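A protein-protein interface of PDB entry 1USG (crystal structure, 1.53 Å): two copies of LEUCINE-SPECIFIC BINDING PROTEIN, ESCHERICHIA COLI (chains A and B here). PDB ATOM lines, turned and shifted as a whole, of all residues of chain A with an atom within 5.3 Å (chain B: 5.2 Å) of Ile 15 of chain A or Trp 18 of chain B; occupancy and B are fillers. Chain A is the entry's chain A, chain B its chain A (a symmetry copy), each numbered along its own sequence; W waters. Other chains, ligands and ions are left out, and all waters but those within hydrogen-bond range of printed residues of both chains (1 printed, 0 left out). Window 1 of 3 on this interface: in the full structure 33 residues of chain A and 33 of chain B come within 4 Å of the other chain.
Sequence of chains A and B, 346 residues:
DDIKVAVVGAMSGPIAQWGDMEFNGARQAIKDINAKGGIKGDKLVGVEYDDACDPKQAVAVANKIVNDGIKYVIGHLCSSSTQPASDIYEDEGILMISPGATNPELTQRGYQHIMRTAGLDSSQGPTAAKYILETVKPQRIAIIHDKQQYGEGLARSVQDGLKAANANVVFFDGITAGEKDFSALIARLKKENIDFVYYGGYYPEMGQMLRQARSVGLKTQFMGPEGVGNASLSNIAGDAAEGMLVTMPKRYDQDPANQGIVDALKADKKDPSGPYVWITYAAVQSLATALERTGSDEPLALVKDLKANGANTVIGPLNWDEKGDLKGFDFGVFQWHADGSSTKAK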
ATOM      1  N   ALA A  10      24.253 -11.766  16.632  1.00  0.00           N
ATOM      2  CA  ALA A  10      23.886 -11.778  18.057  1.00  0.00           C
ATOM      3  C   ALA A  10      22.402 -11.497  18.285  1.00  0.00           C
ATOM      4  O   ALA A  10      21.956 -10.373  18.082  1.00  0.00           O
ATOM      5  CB  ALA A  10      24.722 -10.741  18.797  1.00  0.00           C
ATOM      6  N   SER A  12      21.480 -12.371  21.330  1.00  0.00           N
ATOM      7  CA  SER A  12      21.650 -12.316  22.773  1.00  0.00           C
ATOM      8  C   SER A  12      23.037 -11.818  23.070  1.00  0.00           C
ATOM      9  O   SER A  12      23.880 -11.736  22.192  1.00  0.00           O
ATOM     10  CB  SER A  12      21.445 -13.676  23.393  1.00  0.00           C
ATOM     11  OG  SER A  12      22.469 -14.582  23.019  1.00  0.00           O
ATOM     12  N   GLY A  13      23.266 -11.488  24.328  1.00  0.00           N
ATOM     13  CA  GLY A  13      24.547 -10.948  24.725  1.00  0.00           C
ATOM     14  C   GLY A  13      24.694  -9.473  24.459  1.00  0.00           C
ATOM     15  O   GLY A  13      23.761  -8.759  24.055  1.00  0.00           O
ATOM     16  N   PRO A  14      25.885  -8.964  24.738  1.00  0.00           N
ATOM     17  CA  PRO A  14      26.136  -7.520  24.693  1.00  0.00           C
ATOM     18  C   PRO A  14      26.071  -6.848  23.325  1.00  0.00           C
ATOM     19  O   PRO A  14      25.982  -5.623  23.209  1.00  0.00           O
ATOM     20  CB  PRO A  14      27.530  -7.372  25.313  1.00  0.00           C
ATOM     21  CG  PRO A  14      28.072  -8.728  25.449  1.00  0.00           C
ATOM     22  CD  PRO A  14      27.044  -9.741  25.250  1.00  0.00           C
ATOM     23  N   ILE A  15      26.149  -7.648  22.263  1.00  0.00           N
ATOM     24  CA  ILE A  15      26.090  -7.138  20.890  1.00  0.00           C
ATOM     25  C   ILE A  15      24.689  -7.333  20.251  1.00  0.00           C
ATOM     26  O   ILE A  15      24.525  -7.148  19.048  1.00  0.00           O
ATOM     27  CB  ILE A  15      27.170  -7.837  20.017  1.00  0.00           C
ATOM     28  CG1 ILE A  15      28.524  -8.016  20.748  1.00  0.00           C
ATOM     29  CG2 ILE A  15      27.371  -7.039  18.742  1.00  0.00           C
ATOM     30  CD1 ILE A  15      29.175  -6.748  21.260  1.00  0.00           C
ATOM     31  N   ALA A  16      23.679  -7.624  21.053  1.00  0.00           N
ATOM     32  CA  ALA A  16      22.334  -7.911  20.532  1.00  0.00           C
ATOM     33  C   ALA A  16      21.688  -6.725  19.839  1.00  0.00           C
ATOM     34  O   ALA A  16      20.882  -6.936  18.946  1.00  0.00           O
ATOM     35  CB  ALA A  16      21.413  -8.417  21.646  1.00  0.00           C
ATOM     36  N   GLN A  17      22.019  -5.509  20.217  1.00  0.00           N
ATOM     37  CA  GLN A  17      21.424  -4.369  19.544  1.00  0.00           C
ATOM     38  C   GLN A  17      21.878  -4.277  18.095  1.00  0.00           C
ATOM     39  O   GLN A  17      21.071  -4.013  17.186  1.00  0.00           O
ATOM     40  CB  GLN A  17      21.710  -3.056  20.286  1.00  0.00           C
ATOM     41  CG  GLN A  17      21.074  -3.057  21.659  1.00  0.00           C
ATOM     42  CD  GLN A  17      21.087  -1.697  22.361  1.00  0.00           C
ATOM     43  OE1 GLN A  17      21.910  -0.824  22.047  1.00  0.00           O
ATOM     44  NE2 GLN A  17      20.166  -1.516  23.315  1.00  0.00           N
ATOM     45  N   TRP A  18      23.151  -4.508  17.835  1.00  0.00           N
ATOM     46  CA  TRP A  18      23.654  -4.563  16.470  1.00  0.00           C
ATOM     47  C   TRP A  18      23.174  -5.806  15.748  1.00  0.00           C
ATOM     48  O   TRP A  18      22.898  -5.771  14.541  1.00  0.00           O
ATOM     49  CB  TRP A  18      25.200  -4.501  16.445  1.00  0.00           C
ATOM     50  CG  TRP A  18      25.731  -3.128  16.860  1.00  0.00           C
ATOM     51  CD1 TRP A  18      25.006  -2.068  17.324  1.00  0.00           C
ATOM     52  CD2 TRP A  18      27.081  -2.682  16.769  1.00  0.00           C
ATOM     53  NE1 TRP A  18      25.839  -1.001  17.586  1.00  0.00           N
ATOM     54  CE2 TRP A  18      27.119  -1.344  17.235  1.00  0.00           C
ATOM     55  CE3 TRP A  18      28.273  -3.278  16.325  1.00  0.00           C
ATOM     56  CZ2 TRP A  18      28.291  -0.603  17.278  1.00  0.00           C
ATOM     57  CZ3 TRP A  18      29.432  -2.544  16.367  1.00  0.00           C
ATOM     58  CH2 TRP A  18      29.438  -1.220  16.859  1.00  0.00           C
ATOM     59  N   GLY A  19      23.086  -6.922  16.458  1.00  0.00           N
ATOM     60  CA  GLY A  19      22.529  -8.122  15.852  1.00  0.00           C
ATOM     61  C   GLY A  19      21.097  -7.871  15.387  1.00  0.00           C
ATOM     62  O   GLY A  19      20.690  -8.332  14.316  1.00  0.00           O
ATOM     63  N   ASP A  20      20.283  -7.176  16.180  1.00  0.00           N
ATOM     64  CA  ASP A  20      18.904  -6.894  15.742  1.00  0.00           C
ATOM     65  C   ASP A  20      18.876  -6.112  14.430  1.00  0.00           C
ATOM     66  O   ASP A  20      18.090  -6.400  13.567  1.00  0.00           O
ATOM     67  CB  ASP A  20      18.150  -6.126  16.842  1.00  0.00           C
ATOM     68  CG  ASP A  20      16.665  -6.040  16.608  1.00  0.00           C
ATOM     69  OD1 ASP A  20      15.991  -7.079  16.631  1.00  0.00           O
ATOM     70  OD2 ASP A  20      16.108  -4.946  16.376  1.00  0.00           O
ATOM     71  N   CYS A  53      27.795 -13.584  19.489  1.00  0.00           N
ATOM     72  CA  CYS A  53      29.151 -13.084  19.306  1.00  0.00           C
ATOM     73  C   CYS A  53      30.153 -13.791  20.249  1.00  0.00           C
ATOM     74  O   CYS A  53      31.005 -13.154  20.853  1.00  0.00           O
ATOM     75  CB  CYS A  53      29.145 -11.557  19.499  1.00  0.00           C
ATOM     76  SG  CYS A  53      28.658 -10.680  17.973  1.00  0.00           S
ATOM     77  N   LEU A  77      28.798 -11.535  12.887  1.00  0.00           N
ATOM     78  CA  LEU A  77      28.764 -10.096  13.147  1.00  0.00           C
ATOM     79  C   LEU A  77      30.061  -9.530  13.752  1.00  0.00           C
ATOM     80  O   LEU A  77      30.423  -8.375  13.478  1.00  0.00           O
ATOM     81  CB  LEU A  77      27.563  -9.772  14.061  1.00  0.00           C
ATOM     82  CG  LEU A  77      27.254  -8.295  14.386  1.00  0.00           C
ATOM     83  CD1 LEU A  77      26.936  -7.467  13.139  1.00  0.00           C
ATOM     84  CD2 LEU A  77      26.142  -8.198  15.412  1.00  0.00           C
ATOM     85  N   CYS A  78      30.712 -10.322  14.589  1.00  0.00           N
ATOM     86  CA  CYS A  78      31.890  -9.955  15.374  1.00  0.00           C
ATOM     87  C   CYS A  78      33.081 -10.742  14.895  1.00  0.00           C
ATOM     88  O   CYS A  78      32.919 -11.868  14.441  1.00  0.00           O
ATOM     89  CB  CYS A  78      31.667 -10.348  16.825  1.00  0.00           C
ATOM     90  SG  CYS A  78      30.296  -9.472  17.647  1.00  0.00           S
ATOM     91  N   ILE B  15      34.123   0.346  16.234  1.00  0.00           N
ATOM     92  CA  ILE B  15      33.765   0.287  17.656  1.00  0.00           C
ATOM     93  C   ILE B  15      34.145   1.589  18.410  1.00  0.00           C
ATOM     94  O   ILE B  15      34.101   1.629  19.637  1.00  0.00           O
ATOM     95  CB  ILE B  15      34.457  -0.933  18.326  1.00  0.00           C
ATOM     96  CG1 ILE B  15      34.442  -2.205  17.443  1.00  0.00           C
ATOM     97  CG2 ILE B  15      33.782  -1.217  19.656  1.00  0.00           C
ATOM     98  CD1 ILE B  15      33.077  -2.699  17.012  1.00  0.00           C
ATOM     99  N   ALA B  16      34.436   2.659  17.691  1.00  0.00           N
ATOM    100  CA  ALA B  16      34.889   3.912  18.313  1.00  0.00           C
ATOM    101  C   ALA B  16      33.842   4.560  19.199  1.00  0.00           C
ATOM    102  O   ALA B  16      34.212   5.243  20.142  1.00  0.00           O
ATOM    103  CB  ALA B  16      35.353   4.913  17.251  1.00  0.00           C
ATOM    104  N   GLN B  17      32.568   4.365  18.929  1.00  0.00           N
ATOM    105  CA  GLN B  17      31.560   4.962  19.784  1.00  0.00           C
ATOM    106  C   GLN B  17      31.581   4.355  21.179  1.00  0.00           C
ATOM    107  O   GLN B  17      31.483   5.071  22.192  1.00  0.00           O
ATOM    108  CB  GLN B  17      30.157   4.859  19.169  1.00  0.00           C
ATOM    109  CG  GLN B  17      30.070   5.644  17.879  1.00  0.00           C
ATOM    110  CD  GLN B  17      28.648   5.811  17.338  1.00  0.00           C
ATOM    111  OE1 GLN B  17      27.746   5.023  17.661  1.00  0.00           O
ATOM    112  NE2 GLN B  17      28.447   6.844  16.511  1.00  0.00           N
ATOM    113  N   TRP B  18      31.729   3.048  21.277  1.00  0.00           N
ATOM    114  CA  TRP B  18      31.883   2.391  22.567  1.00  0.00           C
ATOM    115  C   TRP B  18      33.230   2.694  23.190  1.00  0.00           C
ATOM    116  O   TRP B  18      33.345   2.834  24.416  1.00  0.00           O
ATOM    117  CB  TRP B  18      31.692   0.861  22.438  1.00  0.00           C
ATOM    118  CG  TRP B  18      30.243   0.482  22.127  1.00  0.00           C
ATOM    119  CD1 TRP B  18      29.205   1.331  21.865  1.00  0.00           C
ATOM    120  CD2 TRP B  18      29.695  -0.832  22.127  1.00  0.00           C
ATOM    121  NE1 TRP B  18      28.050   0.613  21.639  1.00  0.00           N
ATOM    122  CE2 TRP B  18      28.317  -0.720  21.814  1.00  0.00           C
ATOM    123  CE3 TRP B  18      30.230  -2.108  22.374  1.00  0.00           C
ATOM    124  CZ2 TRP B  18      27.479  -1.821  21.733  1.00  0.00           C
ATOM    125  CZ3 TRP B  18      29.399  -3.198  22.295  1.00  0.00           C
ATOM    126  CH2 TRP B  18      28.035  -3.051  21.958  1.00  0.00           C
ATOM    127  N   GLY B  19      34.269   2.779  22.372  1.00  0.00           N
ATOM    128  CA  GLY B  19      35.569   3.174  22.893  1.00  0.00           C
ATOM    129  C   GLY B  19      35.492   4.559  23.530  1.00  0.00           C
ATOM    130  O   GLY B  19      36.095   4.807  24.579  1.00  0.00           O
ATOM    131  N   ASP B  20      34.790   5.506  22.911  1.00  0.00           N
ATOM    132  CA  ASP B  20      34.673   6.844  23.519  1.00  0.00           C
ATOM    133  C   ASP B  20      34.038   6.781  24.906  1.00  0.00           C
ATOM    134  O   ASP B  20      34.480   7.441  25.808  1.00  0.00           O
ATOM    135  CB  ASP B  20      33.862   7.772  22.597  1.00  0.00           C
ATOM    136  CG  ASP B  20      33.928   9.223  22.993  1.00  0.00           C
ATOM    137  OD1 ASP B  20      35.013   9.818  22.923  1.00  0.00           O
ATOM    138  OD2 ASP B  20      32.916   9.829  23.404  1.00  0.00           O
ATOM    139  N   MET B  21      33.029   5.945  25.077  1.00  0.00           N
ATOM    140  CA  MET B  21      32.391   5.698  26.369  1.00  0.00           C
ATOM    141  C   MET B  21      33.443   5.227  27.403  1.00  0.00           C
ATOM    142  O   MET B  21      33.577   5.758  28.509  1.00  0.00           O
ATOM    143  CB  MET B  21      31.324   4.630  26.265  1.00  0.00           C
ATOM    144  CG  MET B  21      30.188   4.977  25.397  1.00  0.00           C
ATOM    145  SD  MET B  21      29.103   3.544  25.301  1.00  0.00           S
ATOM    146  CE  MET B  21      27.936   4.108  24.064  1.00  0.00           C
ATOM    147  N   GLU B  22      34.223   4.235  26.989  1.00  0.00           N
ATOM    148  CA  GLU B  22      35.297   3.693  27.818  1.00  0.00           C
ATOM    149  C   GLU B  22      36.296   4.776  28.236  1.00  0.00           C
ATOM    150  O   GLU B  22      36.581   4.898  29.430  1.00  0.00           O
ATOM    151  CB  GLU B  22      35.962   2.534  27.050  1.00  0.00           C
ATOM    152  CG  GLU B  22      37.148   1.914  27.770  1.00  0.00           C
ATOM    153  CD  GLU B  22      38.034   1.035  26.907  1.00  0.00           C
ATOM    154  OE1 GLU B  22      37.816   0.934  25.692  1.00  0.00           O
ATOM    155  OE2 GLU B  22      38.962   0.427  27.504  1.00  0.00           O
ATOM    156  N   LEU B  77      38.726  -3.623  24.785  1.00  0.00           N
ATOM    157  CA  LEU B  77      37.275  -3.454  24.693  1.00  0.00           C
ATOM    158  C   LEU B  77      36.540  -4.630  24.024  1.00  0.00           C
ATOM    159  O   LEU B  77      35.394  -4.935  24.388  1.00  0.00           O
ATOM    160  CB  LEU B  77      36.961  -2.137  23.953  1.00  0.00           C
ATOM    161  CG  LEU B  77      35.490  -1.686  23.830  1.00  0.00           C
ATOM    162  CD1 LEU B  77      34.827  -1.450  25.188  1.00  0.00           C
ATOM    163  CD2 LEU B  77      35.383  -0.460  22.944  1.00  0.00           C
ATOM    164  N   THR B 102      32.030  -9.539  25.884  1.00  0.00           N
ATOM    165  CA  THR B 102      31.851 -10.760  25.116  1.00  0.00           C
ATOM    166  C   THR B 102      32.903 -11.804  25.518  1.00  0.00           C
ATOM    167  O   THR B 102      33.878 -11.497  26.187  1.00  0.00           O
ATOM    168  CB  THR B 102      31.909 -10.451  23.603  1.00  0.00           C
ATOM    169  OG1 THR B 102      33.252 -10.135  23.230  1.00  0.00           O
ATOM    170  CG2 THR B 102      31.115  -9.179  23.265  1.00  0.00           C
ATOM    171  N   TYR B 276      29.332   1.272  28.876  1.00  0.00           N
ATOM    172  CA  TYR B 276      30.799   1.203  29.005  1.00  0.00           C
ATOM    173  C   TYR B 276      31.401   2.397  29.741  1.00  0.00           C
ATOM    174  O   TYR B 276      32.502   2.302  30.266  1.00  0.00           O
ATOM    175  CB  TYR B 276      31.466   0.928  27.640  1.00  0.00           C
ATOM    176  CG  TYR B 276      30.919  -0.355  27.087  1.00  0.00           C
ATOM    177  CD1 TYR B 276      29.911  -0.380  26.143  1.00  0.00           C
ATOM    178  CD2 TYR B 276      31.322  -1.555  27.634  1.00  0.00           C
ATOM    179  CE1 TYR B 276      29.318  -1.620  25.748  1.00  0.00           C
ATOM    180  CE2 TYR B 276      30.746  -2.759  27.259  1.00  0.00           C
ATOM    181  CZ  TYR B 276      29.772  -2.795  26.306  1.00  0.00           C
ATOM    182  OH  TYR B 276      29.213  -4.008  25.919  1.00  0.00           O
HETATM  183  O   HOH W   1      26.465  -4.024  25.392  1.00  0.00           O
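The side-chain sulfur of Cys 78 of chain A forms a disulfide with the side-chain sulfur of Cys 53 of chain A, at 2.1 Å.
Among the printed residues, merely in contact across the chains: Pro 14 of chain A with Trp 18 of chain B, Pro 14 of chain A with Thr 102 of chain B, Pro 14 of chain A with Tyr 276 of chain B, Ile 15 of chain A with Trp 18 of chain B, Ile 15 of chain A with Thr 102 of chain B, Trp 18 of chain A with Ile 15 of chain B and Cys 53 of chain A with Thr 102 of chain B.
Of chain B, only Trp 18 (3.7 Å) and Thr 102 (3.7 Å) come within 4 Å of Ile 15 of chain A. Trp 18 of chain B touches just these residues of chain A: Pro 14 (3.5 Å) and Ile 15 (3.7 Å). Printed residues of chain B within 4 Å of Cys 53 of chain A: Thr 102. Of the printed residues of chain A, Ile 15 of chain B touches Trp 18. Printed residues of chain A within 4 Å of Tyr 276 of chain B: Pro 14 (3.8 Å). Of the printed residues of chain A, Thr 102 of chain B touches Pro 14, Ile 15 and Cys 53. Printed residues of chain B within 4 Å of Pro 14 of chain A: Trp 18 (3.5 Å), Thr 102 (3.8 Å) and Tyr 276 (3.8 Å). Ala 16 of chain B touches none of the printed residues of chain A. The nearest printed residue of chain B that does not touch Ile 15 of chain A is Tyr 276 of chain B (5.4 Å).
Hydrophobic or aromatic side chains of chain B that line the printed part of chain A: Ile 15, Trp 18 and Tyr 276. Printed residues of chain A that touch a printed residue of chain B: Pro 14, Ile 15, Trp 18 and Cys 53.
Ile 15 of chain A touches Trp 18 of chain B, and with the chains exchanged Trp 18 of chain A touches Ile 15 of chain B. Positions printed for both chains: 15, 16, 17, 18, 19, 20 and 77. Of the 7 pairs that touch across the chains among the printed residues, 2 have their exchanged pair printed and touching as well.
Water W1 bridges O of Pro 14 of chain A (2.7 Å) and OH of Tyr 276 of chain B (2.8 Å).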
